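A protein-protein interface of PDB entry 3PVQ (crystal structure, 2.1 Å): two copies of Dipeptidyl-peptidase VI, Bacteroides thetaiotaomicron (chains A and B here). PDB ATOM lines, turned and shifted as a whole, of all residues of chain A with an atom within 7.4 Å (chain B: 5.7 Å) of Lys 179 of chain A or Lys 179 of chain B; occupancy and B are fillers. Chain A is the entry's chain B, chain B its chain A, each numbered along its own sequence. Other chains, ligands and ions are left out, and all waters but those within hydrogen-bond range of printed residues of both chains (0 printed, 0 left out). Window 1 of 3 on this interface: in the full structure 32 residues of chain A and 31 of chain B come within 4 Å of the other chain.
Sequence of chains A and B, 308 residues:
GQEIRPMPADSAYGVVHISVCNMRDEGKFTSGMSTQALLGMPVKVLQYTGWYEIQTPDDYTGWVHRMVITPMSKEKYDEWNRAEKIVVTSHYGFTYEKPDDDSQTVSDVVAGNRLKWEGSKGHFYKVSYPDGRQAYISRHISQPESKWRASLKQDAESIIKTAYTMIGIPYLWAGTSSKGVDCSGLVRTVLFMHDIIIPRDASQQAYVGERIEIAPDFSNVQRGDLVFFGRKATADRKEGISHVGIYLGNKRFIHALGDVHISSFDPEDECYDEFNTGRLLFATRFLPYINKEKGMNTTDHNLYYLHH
Of chain B, only Tyr 92 (3.7 Å) and Lys 179 (2.7 Å) come within 4 Å of Lys 179 of chain A. Printed residues of chain A within 4 Å of Tyr 92 of chain B: Tyr 92, Asp 108 and Lys 179. Of the printed residues of chain A, Val 20 of chain B touches Pro 170 (3.6 Å). His 91 of chain A touches none of the printed residues of chain B. Ser 178 of chain B touches none of the printed residues of chain A. The nearest residue of chain A that does not touch Lys 179 of chain B is Pro 170 of chain A (4.3 Å).
The side-chain carboxylate of Asp 108 of chain B lies within salt-bridge range of the side-chain amino group of Lys 179 of chain B, 2.8 Å away. The backbone carbonyl oxygen of Pro 170 of chain B sits at hydrogen-bond distance from the backbone NH of Val 181 of chain B (3.1 Å). The backbone NH of Leu 172 of chain B sits at hydrogen-bond distance from the backbone carbonyl oxygen of Val 181 of chain B, 2.9 Å away. The side-chain hydroxyl (OG) of Ser 177 of chain B sits close to the backbone NH (N) of Lys 179 of chain B. The backbone carbonyl oxygen of Ser 19 of chain A sits at hydrogen-bond distance from the side-chain amide nitrogen of Asn 113 of chain A, at 2.8 Å. The backbone carbonyl oxygen of Pro 170 of chain A lies within hydrogen-bond range of the backbone NH of Val 181 of chain A.
The backbone carbonyl oxygen of Lys 179 of chain A is in hydrogen-bond range of the side-chain amino group of Lys 179 of chain B (2.7 Å).
Ser 19 of chain A touches Pro 170 of chain B, and with the chains exchanged Pro 170 of chain A touches Ser 19 of chain B. Val 20 of chain A touches Pro 170 of chain B, and with the chains exchanged Pro 170 of chain A touches Val 20 of chain B. Tyr 92 of chain B touches its own counterpart, Tyr 92 of chain A. Tyr 92 of chain A touches Asp 108 of chain B, and with the chains exchanged Asp 108 of chain A touches Tyr 92 of chain B. 13 positions are printed for both chains.
Along chain A the printed residues that touch a printed residue of chain B span positions 19 to 179. Hydrophobic or aromatic side chains of chain B that line the printed part of chain A: Tyr 92, Ile 169, Pro 170 and Leu 172. Among the printed residues, 15 pairs touch across the chains. Among the printed residues, no Asp or Glu carboxylate lies within 4 Å of a Lys or Arg side-chain nitrogen of the other chain.
OG of Ser 19 of chain A touches CG of Pro 170 of chain B, 3.2 Å away. O of Val 20 of chain A touches CB of Pro 170 of chain B, at 3.6 Å. Tyr 92 of chain B touches Tyr 92 of chain A. OH of Tyr 92 of chain A touches CB of Asp 108 of chain B (3.6 Å). Lys 179 of chain B touches Tyr 92 of chain A (NZ to OH, 3.7 Å). Ile 169 of chain B touches Asp 108 of chain A (CA to OD1, 3.4 Å). OD1 of Asp 108 of chain B touches CA of Ile 169 of chain A, 3.4 Å away. Pro 170 of chain A touches Ser 19 of chain B. Pro 170 of chain A touches Val 20 of chain B (CB to O, 3.6 Å). Tyr 92 of chain B touches Lys 179 of chain A (OH to NZ, 3.7 Å).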
ATOM      1  N   SER A  19      24.795  19.501  18.660  1.00  0.00           N
ATOM      2  CA  SER A  19      23.873  19.416  19.825  1.00  0.00           C
ATOM      3  C   SER A  19      23.689  20.769  20.540  1.00  0.00           C
ATOM      4  O   SER A  19      22.550  21.177  20.800  1.00  0.00           O
ATOM      5  CB  SER A  19      24.335  18.369  20.827  1.00  0.00           C
ATOM      6  OG  SER A  19      25.590  18.725  21.401  1.00  0.00           O
ATOM      7  N   VAL A  20      24.814  21.458  20.836  1.00  0.00           N
ATOM      8  CA  VAL A  20      24.857  22.760  21.518  1.00  0.00           C
ATOM      9  C   VAL A  20      25.964  23.602  20.880  1.00  0.00           C
ATOM     10  O   VAL A  20      27.126  23.177  20.877  1.00  0.00           O
ATOM     11  CB  VAL A  20      25.094  22.614  23.065  1.00  0.00           C
ATOM     12  CG1 VAL A  20      25.116  23.972  23.742  1.00  0.00           C
ATOM     13  CG2 VAL A  20      24.050  21.714  23.726  1.00  0.00           C
ATOM     14  N   CYS A  21      25.630  24.798  20.383  1.00  0.00           N
ATOM     15  CA  CYS A  21      26.689  25.651  19.843  1.00  0.00           C
ATOM     16  C   CYS A  21      26.897  26.800  20.798  1.00  0.00           C
ATOM     17  O   CYS A  21      26.020  27.074  21.607  1.00  0.00           O
ATOM     18  CB  CYS A  21      26.421  26.102  18.408  1.00  0.00           C
ATOM     19  SG  CYS A  21      25.148  27.363  18.254  1.00  0.00           S
ATOM     20  N   ASN A  22      28.089  27.380  20.798  1.00  0.00           N
ATOM     21  CA  ASN A  22      28.512  28.384  21.779  1.00  0.00           C
ATOM     22  C   ASN A  22      28.623  29.752  21.164  1.00  0.00           C
ATOM     23  O   ASN A  22      29.569  30.018  20.428  1.00  0.00           O
ATOM     24  CB  ASN A  22      29.863  27.931  22.410  1.00  0.00           C
ATOM     25  CG  ASN A  22      29.871  26.453  22.743  1.00  0.00           C
ATOM     26  OD1 ASN A  22      29.011  25.953  23.466  1.00  0.00           O
ATOM     27  ND2 ASN A  22      30.720  25.685  22.091  1.00  0.00           N
ATOM     28  N   GLN A  36      23.838  30.059  24.181  1.00  0.00           N
ATOM     29  CA  GLN A  36      23.995  28.827  23.400  1.00  0.00           C
ATOM     30  C   GLN A  36      22.745  28.541  22.617  1.00  0.00           C
ATOM     31  O   GLN A  36      21.670  28.898  23.080  1.00  0.00           O
ATOM     32  CB  GLN A  36      24.318  27.643  24.323  1.00  0.00           C
ATOM     33  CG  GLN A  36      25.706  27.740  24.931  1.00  0.00           C
ATOM     34  CD  GLN A  36      26.004  26.609  25.863  1.00  0.00           C
ATOM     35  OE1 GLN A  36      25.135  26.139  26.577  1.00  0.00           O
ATOM     36  NE2 GLN A  36      27.227  26.089  25.811  1.00  0.00           N
ATOM     37  N   HIS A  91      17.589  14.411  28.801  1.00  0.00           N
ATOM     38  CA  HIS A  91      18.685  15.378  28.948  1.00  0.00           C
ATOM     39  C   HIS A  91      19.856  15.049  28.025  1.00  0.00           C
ATOM     40  O   HIS A  91      20.347  15.946  27.344  1.00  0.00           O
ATOM     41  CB  HIS A  91      19.183  15.488  30.406  1.00  0.00           C
ATOM     42  CG  HIS A  91      18.216  16.244  31.281  1.00  0.00           C
ATOM     43  ND1 HIS A  91      17.861  17.550  30.999  1.00  0.00           N
ATOM     44  CD2 HIS A  91      17.534  15.838  32.374  1.00  0.00           C
ATOM     45  CE1 HIS A  91      16.985  17.896  31.929  1.00  0.00           C
ATOM     46  NE2 HIS A  91      16.774  16.905  32.788  1.00  0.00           N
ATOM     47  N   TYR A  92      20.305  13.780  28.004  1.00  0.00           N
ATOM     48  CA  TYR A  92      21.484  13.361  27.245  1.00  0.00           C
ATOM     49  C   TYR A  92      21.240  12.102  26.461  1.00  0.00           C
ATOM     50  O   TYR A  92      20.459  11.249  26.876  1.00  0.00           O
ATOM     51  CB  TYR A  92      22.688  13.107  28.206  1.00  0.00           C
ATOM     52  CG  TYR A  92      22.901  14.180  29.254  1.00  0.00           C
ATOM     53  CD1 TYR A  92      23.086  15.515  28.890  1.00  0.00           C
ATOM     54  CD2 TYR A  92      22.959  13.859  30.605  1.00  0.00           C
ATOM     55  CE1 TYR A  92      23.300  16.503  29.852  1.00  0.00           C
ATOM     56  CE2 TYR A  92      23.173  14.838  31.571  1.00  0.00           C
ATOM     57  CZ  TYR A  92      23.318  16.164  31.194  1.00  0.00           C
ATOM     58  OH  TYR A  92      23.526  17.133  32.160  1.00  0.00           O
ATOM     59  N   GLY A  93      21.990  11.960  25.377  1.00  0.00           N
ATOM     60  CA  GLY A  93      21.955  10.758  24.554  1.00  0.00           C
ATOM     61  C   GLY A  93      22.817  10.867  23.331  1.00  0.00           C
ATOM     62  O   GLY A  93      23.570  11.832  23.177  1.00  0.00           O
ATOM     63  N   ASP A 108      26.273  13.399  19.862  1.00  0.00           N
ATOM     64  CA  ASP A 108      25.532  13.437  21.104  1.00  0.00           C
ATOM     65  C   ASP A 108      24.259  14.281  20.809  1.00  0.00           C
ATOM     66  O   ASP A 108      24.195  15.002  19.794  1.00  0.00           O
ATOM     67  CB  ASP A 108      26.371  14.071  22.224  1.00  0.00           C
ATOM     68  CG  ASP A 108      26.673  15.537  21.937  1.00  0.00           C
ATOM     69  OD1 ASP A 108      27.127  15.839  20.803  1.00  0.00           O
ATOM     70  OD2 ASP A 108      26.315  16.389  22.780  1.00  0.00           O
ATOM     71  N   VAL A 109      23.281  14.212  21.693  1.00  0.00           N
ATOM     72  CA  VAL A 109      22.091  15.048  21.645  1.00  0.00           C
ATOM     73  C   VAL A 109      21.799  15.485  23.056  1.00  0.00           C
ATOM     74  O   VAL A 109      22.250  14.829  23.992  1.00  0.00           O
ATOM     75  CB  VAL A 109      20.855  14.376  20.988  1.00  0.00           C
ATOM     76  CG1 VAL A 109      21.067  14.154  19.482  1.00  0.00           C
ATOM     77  CG2 VAL A 109      20.447  13.078  21.707  1.00  0.00           C
ATOM     78  N   VAL A 110      21.063  16.591  23.217  1.00  0.00           N
ATOM     79  CA  VAL A 110      20.565  17.060  24.503  1.00  0.00           C
ATOM     80  C   VAL A 110      19.081  17.352  24.313  1.00  0.00           C
ATOM     81  O   VAL A 110      18.646  17.522  23.171  1.00  0.00           O
ATOM     82  CB  VAL A 110      21.317  18.284  25.127  1.00  0.00           C
ATOM     83  CG1 VAL A 110      22.767  17.946  25.459  1.00  0.00           C
ATOM     84  CG2 VAL A 110      21.221  19.526  24.255  1.00  0.00           C
ATOM     85  N   ALA A 111      18.314  17.439  25.412  1.00  0.00           N
ATOM     86  CA  ALA A 111      16.896  17.823  25.367  1.00  0.00           C
ATOM     87  C   ALA A 111      16.744  19.139  24.610  1.00  0.00           C
ATOM     88  O   ALA A 111      17.590  20.031  24.765  1.00  0.00           O
ATOM     89  CB  ALA A 111      16.362  17.969  26.795  1.00  0.00           C
ATOM     90  N   ASN A 113      16.976  19.412  21.343  1.00  0.00           N
ATOM     91  CA  ASN A 113      17.490  19.146  19.996  1.00  0.00           C
ATOM     92  C   ASN A 113      16.348  18.660  19.122  1.00  0.00           C
ATOM     93  O   ASN A 113      15.448  17.961  19.616  1.00  0.00           O
ATOM     94  CB  ASN A 113      18.600  18.098  20.041  1.00  0.00           C
ATOM     95  CG  ASN A 113      19.954  18.580  20.487  1.00  0.00           C
ATOM     96  OD1 ASN A 113      20.902  17.851  20.407  1.00  0.00           O
ATOM     97  ND2 ASN A 113      20.098  19.809  20.953  1.00  0.00           N
ATOM     98  N   MET A 166      16.987  18.478  36.842  1.00  0.00           N
ATOM     99  CA  MET A 166      18.242  19.172  36.542  1.00  0.00           C
ATOM    100  C   MET A 166      19.117  19.446  37.781  1.00  0.00           C
ATOM    101  O   MET A 166      20.183  20.062  37.651  1.00  0.00           O
ATOM    102  CB  MET A 166      17.908  20.472  35.827  1.00  0.00           C
ATOM    103  CG  MET A 166      17.318  20.175  34.431  1.00  0.00           C
ATOM    104  SD  MET A 166      17.452  21.656  33.254  1.00  0.00           S
ATOM    105  CE  MET A 166      19.344  21.760  33.104  1.00  0.00           C
ATOM    106  N   ILE A 169      23.270  19.608  38.204  1.00  0.00           N
ATOM    107  CA  ILE A 169      23.890  19.924  36.915  1.00  0.00           C
ATOM    108  C   ILE A 169      24.756  21.172  37.133  1.00  0.00           C
ATOM    109  O   ILE A 169      24.336  22.048  37.897  1.00  0.00           O
ATOM    110  CB  ILE A 169      22.840  20.066  35.782  1.00  0.00           C
ATOM    111  CG1 ILE A 169      22.369  18.658  35.328  1.00  0.00           C
ATOM    112  CG2 ILE A 169      23.352  20.893  34.593  1.00  0.00           C
ATOM    113  CD1 ILE A 169      21.162  18.672  34.386  1.00  0.00           C
ATOM    114  N   PRO A 170      25.966  21.246  36.531  1.00  0.00           N
ATOM    115  CA  PRO A 170      26.830  22.388  36.793  1.00  0.00           C
ATOM    116  C   PRO A 170      26.324  23.723  36.320  1.00  0.00           C
ATOM    117  O   PRO A 170      25.631  23.826  35.318  1.00  0.00           O
ATOM    118  CB  PRO A 170      28.111  22.052  36.002  1.00  0.00           C
ATOM    119  CG  PRO A 170      28.060  20.638  35.745  1.00  0.00           C
ATOM    120  CD  PRO A 170      26.632  20.294  35.615  1.00  0.00           C
ATOM    121  N   TYR A 171      26.745  24.759  37.032  1.00  0.00           N
ATOM    122  CA  TYR A 171      26.571  26.111  36.577  1.00  0.00           C
ATOM    123  C   TYR A 171      27.607  26.308  35.470  1.00  0.00           C
ATOM    124  O   TYR A 171      28.732  25.831  35.582  1.00  0.00           O
ATOM    125  CB  TYR A 171      26.769  27.115  37.724  1.00  0.00           C
ATOM    126  CG  TYR A 171      26.706  28.563  37.285  1.00  0.00           C
ATOM    127  CD1 TYR A 171      27.807  29.181  36.692  1.00  0.00           C
ATOM    128  CD2 TYR A 171      25.560  29.323  37.486  1.00  0.00           C
ATOM    129  CE1 TYR A 171      27.745  30.504  36.256  1.00  0.00           C
ATOM    130  CE2 TYR A 171      25.511  30.669  37.113  1.00  0.00           C
ATOM    131  CZ  TYR A 171      26.595  31.246  36.471  1.00  0.00           C
ATOM    132  OH  TYR A 171      26.552  32.564  36.086  1.00  0.00           O
ATOM    133  N   LEU A 172      27.241  27.012  34.421  1.00  0.00           N
ATOM    134  CA  LEU A 172      28.135  27.342  33.330  1.00  0.00           C
ATOM    135  C   LEU A 172      27.727  28.691  32.798  1.00  0.00           C
ATOM    136  O   LEU A 172      26.600  28.829  32.320  1.00  0.00           O
ATOM    137  CB  LEU A 172      28.088  26.251  32.238  1.00  0.00           C
ATOM    138  CG  LEU A 172      28.808  26.578  30.939  1.00  0.00           C
ATOM    139  CD1 LEU A 172      30.332  26.533  31.134  1.00  0.00           C
ATOM    140  CD2 LEU A 172      28.396  25.645  29.846  1.00  0.00           C
ATOM    141  N   GLY A 175      25.493  29.213  29.902  1.00  0.00           N
ATOM    142  CA  GLY A 175      25.018  27.846  29.668  1.00  0.00           C
ATOM    143  C   GLY A 175      23.523  27.840  29.391  1.00  0.00           C
ATOM    144  O   GLY A 175      22.738  28.411  30.162  1.00  0.00           O
ATOM    145  N   THR A 176      23.120  27.238  28.267  1.00  0.00           N
ATOM    146  CA  THR A 176      21.715  27.286  27.905  1.00  0.00           C
ATOM    147  C   THR A 176      21.287  25.897  27.447  1.00  0.00           C
ATOM    148  O   THR A 176      20.491  25.785  26.532  1.00  0.00           O
ATOM    149  CB  THR A 176      21.471  28.412  26.868  1.00  0.00           C
ATOM    150  OG1 THR A 176      22.322  29.524  27.190  1.00  0.00           O
ATOM    151  CG2 THR A 176      20.022  28.871  26.827  1.00  0.00           C
ATOM    152  N   SER A 177      21.780  24.832  28.116  1.00  0.00           N
ATOM    153  CA  SER A 177      21.358  23.475  27.755  1.00  0.00           C
ATOM    154  C   SER A 177      21.452  22.570  28.950  1.00  0.00           C
ATOM    155  O   SER A 177      22.018  22.960  29.978  1.00  0.00           O
ATOM    156  CB  SER A 177      22.214  22.924  26.609  1.00  0.00           C
ATOM    157  OG  SER A 177      23.442  22.402  27.115  1.00  0.00           O
ATOM    158  N   SER A 178      21.009  21.304  28.784  1.00  0.00           N
ATOM    159  CA  SER A 178      21.124  20.265  29.834  1.00  0.00           C
ATOM    160  C   SER A 178      22.600  20.027  30.254  1.00  0.00           C
ATOM    161  O   SER A 178      22.837  19.575  31.363  1.00  0.00           O
ATOM    162  CB  SER A 178      20.508  18.956  29.346  1.00  0.00           C
ATOM    163  OG  SER A 178      19.151  19.191  29.014  1.00  0.00           O
ATOM    164  N   LYS A 179      23.574  20.356  29.389  1.00  0.00           N
ATOM    165  CA  LYS A 179      25.017  20.170  29.689  1.00  0.00           C
ATOM    166  C   LYS A 179      25.514  21.035  30.881  1.00  0.00           C
ATOM    167  O   LYS A 179      26.391  20.602  31.628  1.00  0.00           O
ATOM    168  CB  LYS A 179      25.876  20.485  28.465  1.00  0.00           C
ATOM    169  CG  LYS A 179      25.773  19.469  27.327  1.00  0.00           C
ATOM    170  CD  LYS A 179      26.566  19.928  26.102  1.00  0.00           C
ATOM    171  CE  LYS A 179      26.437  19.045  24.880  1.00  0.00           C
ATOM    172  NZ  LYS A 179      27.118  17.729  25.066  1.00  0.00           N
ATOM    173  N   GLY A 180      24.961  22.240  31.033  1.00  0.00           N
ATOM    174  CA  GLY A 180      25.331  23.180  32.097  1.00  0.00           C
ATOM    175  C   GLY A 180      24.557  24.457  31.877  1.00  0.00           C
ATOM    176  O   GLY A 180      24.236  24.780  30.738  1.00  0.00           O
ATOM    177  N   VAL A 181      24.158  25.151  32.945  1.00  0.00           N
ATOM    178  CA  VAL A 181      23.276  26.305  32.790  1.00  0.00           C
ATOM    179  C   VAL A 181      23.693  27.463  33.672  1.00  0.00           C
ATOM    180  O   VAL A 181      24.306  27.249  34.709  1.00  0.00           O
ATOM    181  CB  VAL A 181      21.811  25.889  33.139  1.00  0.00           C
ATOM    182  CG1 VAL A 181      21.145  25.093  32.028  1.00  0.00           C
ATOM    183  CG2 VAL A 181      21.738  25.131  34.460  1.00  0.00           C
ATOM    184  N   THR A 189      16.261  26.657  29.649  1.00  0.00           N
ATOM    185  CA  THR A 189      16.423  25.218  29.351  1.00  0.00           C
ATOM    186  C   THR A 189      15.172  24.459  29.810  1.00  0.00           C
ATOM    187  O   THR A 189      14.662  23.616  29.064  1.00  0.00           O
ATOM    188  CB  THR A 189      17.725  24.688  29.999  1.00  0.00           C
ATOM    189  OG1 THR A 189      18.808  25.464  29.474  1.00  0.00           O
ATOM    190  CG2 THR A 189      18.001  23.225  29.683  1.00  0.00           C
ATOM    191  N   SER B  19      30.128  17.531  38.347  1.00  0.00           N
ATOM    192  CA  SER B  19      30.581  16.673  37.220  1.00  0.00           C
ATOM    193  C   SER B  19      31.777  17.283  36.440  1.00  0.00           C
ATOM    194  O   SER B  19      32.765  16.597  36.187  1.00  0.00           O
ATOM    195  CB  SER B  19      29.437  16.376  36.259  1.00  0.00           C
ATOM    196  OG  SER B  19      28.980  17.556  35.622  1.00  0.00           O
ATOM    197  N   VAL B  20      31.659  18.573  36.069  1.00  0.00           N
ATOM    198  CA  VAL B  20      32.659  19.338  35.314  1.00  0.00           C
ATOM    199  C   VAL B  20      32.692  20.773  35.866  1.00  0.00           C
ATOM    200  O   VAL B  20      31.659  21.467  35.849  1.00  0.00           O
ATOM    201  CB  VAL B  20      32.350  19.351  33.765  1.00  0.00           C
ATOM    202  CG1 VAL B  20      33.424  20.135  32.999  1.00  0.00           C
ATOM    203  CG2 VAL B  20      32.207  17.941  33.194  1.00  0.00           C
ATOM    204  N   TYR B  92      27.917   9.993  29.474  1.00  0.00           N
ATOM    205  CA  TYR B  92      26.911  10.743  30.232  1.00  0.00           C
ATOM    206  C   TYR B  92      26.070   9.848  31.120  1.00  0.00           C
ATOM    207  O   TYR B  92      25.803   8.703  30.770  1.00  0.00           O
ATOM    208  CB  TYR B  92      25.956  11.492  29.263  1.00  0.00           C
ATOM    209  CG  TYR B  92      26.650  12.252  28.154  1.00  0.00           C
ATOM    210  CD1 TYR B  92      27.627  13.207  28.438  1.00  0.00           C
ATOM    211  CD2 TYR B  92      26.343  12.007  26.813  1.00  0.00           C
ATOM    212  CE1 TYR B  92      28.269  13.911  27.418  1.00  0.00           C
ATOM    213  CE2 TYR B  92      26.995  12.694  25.783  1.00  0.00           C
ATOM    214  CZ  TYR B  92      27.952  13.648  26.092  1.00  0.00           C
ATOM    215  OH  TYR B  92      28.616  14.320  25.092  1.00  0.00           O
ATOM    216  N   ASP B 108      24.316  15.062  37.478  1.00  0.00           N
ATOM    217  CA  ASP B 108      24.753  14.403  36.261  1.00  0.00           C
ATOM    218  C   ASP B 108      26.195  13.892  36.544  1.00  0.00           C
ATOM    219  O   ASP B 108      26.823  14.332  37.493  1.00  0.00           O
ATOM    220  CB  ASP B 108      24.736  15.383  35.064  1.00  0.00           C
ATOM    221  CG  ASP B 108      25.736  16.513  35.249  1.00  0.00           C
ATOM    222  OD1 ASP B 108      25.736  17.124  36.323  1.00  0.00           O
ATOM    223  OD2 ASP B 108      26.602  16.684  34.373  1.00  0.00           O
ATOM    224  N   VAL B 110      29.875  12.530  34.104  1.00  0.00           N
ATOM    225  CA  VAL B 110      30.502  12.347  32.804  1.00  0.00           C
ATOM    226  C   VAL B 110      31.614  11.334  33.009  1.00  0.00           C
ATOM    227  O   VAL B 110      32.040  11.140  34.154  1.00  0.00           O
ATOM    228  CB  VAL B 110      31.013  13.644  32.105  1.00  0.00           C
ATOM    229  CG1 VAL B 110      29.874  14.588  31.753  1.00  0.00           C
ATOM    230  CG2 VAL B 110      32.112  14.342  32.904  1.00  0.00           C
ATOM    231  N   ILE B 169      30.559  15.206  18.946  1.00  0.00           N
ATOM    232  CA  ILE B 169      30.477  15.972  20.184  1.00  0.00           C
ATOM    233  C   ILE B 169      30.948  17.392  19.862  1.00  0.00           C
ATOM    234  O   ILE B 169      31.881  17.525  19.076  1.00  0.00           O
ATOM    235  CB  ILE B 169      31.251  15.291  21.343  1.00  0.00           C
ATOM    236  CG1 ILE B 169      30.439  14.108  21.892  1.00  0.00           C
ATOM    237  CG2 ILE B 169      31.650  16.280  22.472  1.00  0.00           C
ATOM    238  CD1 ILE B 169      31.211  13.196  22.859  1.00  0.00           C
ATOM    239  N   PRO B 170      30.307  18.455  20.428  1.00  0.00           N
ATOM    240  CA  PRO B 170      30.692  19.814  20.046  1.00  0.00           C
ATOM    241  C   PRO B 170      32.076  20.223  20.463  1.00  0.00           C
ATOM    242  O   PRO B 170      32.585  19.799  21.494  1.00  0.00           O
ATOM    243  CB  PRO B 170      29.670  20.697  20.783  1.00  0.00           C
ATOM    244  CG  PRO B 170      28.584  19.830  21.132  1.00  0.00           C
ATOM    245  CD  PRO B 170      29.150  18.475  21.351  1.00  0.00           C
ATOM    246  N   LEU B 172      34.270  22.959  22.106  1.00  0.00           N
ATOM    247  CA  LEU B 172      34.072  23.950  23.138  1.00  0.00           C
ATOM    248  C   LEU B 172      35.443  24.435  23.556  1.00  0.00           C
ATOM    249  O   LEU B 172      36.253  23.623  23.958  1.00  0.00           O
ATOM    250  CB  LEU B 172      33.286  23.360  24.339  1.00  0.00           C
ATOM    251  CG  LEU B 172      33.245  24.211  25.625  1.00  0.00           C
ATOM    252  CD1 LEU B 172      32.394  25.473  25.428  1.00  0.00           C
ATOM    253  CD2 LEU B 172      32.709  23.403  26.776  1.00  0.00           C
ATOM    254  N   SER B 177      35.953  17.637  28.776  1.00  0.00           N
ATOM    255  CA  SER B 177      35.089  16.537  29.233  1.00  0.00           C
ATOM    256  C   SER B 177      34.232  16.052  28.099  1.00  0.00           C
ATOM    257  O   SER B 177      34.190  16.672  27.028  1.00  0.00           O
ATOM    258  CB  SER B 177      34.206  17.001  30.397  1.00  0.00           C
ATOM    259  OG  SER B 177      32.987  17.570  29.937  1.00  0.00           O
ATOM    260  N   SER B 178      33.497  14.969  28.335  1.00  0.00           N
ATOM    261  CA  SER B 178      32.586  14.403  27.333  1.00  0.00           C
ATOM    262  C   SER B 178      31.503  15.413  26.864  1.00  0.00           C
ATOM    263  O   SER B 178      30.982  15.271  25.786  1.00  0.00           O
ATOM    264  CB  SER B 178      31.914  13.159  27.898  1.00  0.00           C
ATOM    265  OG  SER B 178      32.918  12.228  28.250  1.00  0.00           O
ATOM    266  N   LYS B 179      31.196  16.438  27.661  1.00  0.00           N
ATOM    267  CA  LYS B 179      30.202  17.471  27.329  1.00  0.00           C
ATOM    268  C   LYS B 179      30.571  18.306  26.086  1.00  0.00           C
ATOM    269  O   LYS B 179      29.668  18.707  25.337  1.00  0.00           O
ATOM    270  CB  LYS B 179      29.996  18.426  28.511  1.00  0.00           C
ATOM    271  CG  LYS B 179      29.273  17.807  29.710  1.00  0.00           C
ATOM    272  CD  LYS B 179      29.184  18.824  30.869  1.00  0.00           C
ATOM    273  CE  LYS B 179      28.597  18.227  32.120  1.00  0.00           C
ATOM    274  NZ  LYS B 179      27.113  18.036  31.981  1.00  0.00           N
ATOM    275  N   GLY B 180      31.871  18.578  25.913  1.00  0.00           N
ATOM    276  CA  GLY B 180      32.398  19.408  24.828  1.00  0.00           C
ATOM    277  C   GLY B 180      33.901  19.535  24.960  1.00  0.00           C
ATOM    278  O   GLY B 180      34.416  19.557  26.077  1.00  0.00           O
ATOM    279  N   VAL B 181      34.639  19.532  23.829  1.00  0.00           N
ATOM    280  CA  VAL B 181      36.110  19.566  23.910  1.00  0.00           C
ATOM    281  C   VAL B 181      36.711  20.538  22.920  1.00  0.00           C
ATOM    282  O   VAL B 181      36.143  20.750  21.852  1.00  0.00           O
ATOM    283  CB  VAL B 181      36.743  18.140  23.680  1.00  0.00           C
ATOM    284  CG1 VAL B 181      36.530  17.198  24.867  1.00  0.00           C
ATOM    285  CG2 VAL B 181      36.256  17.499  22.376  1.00  0.00           C
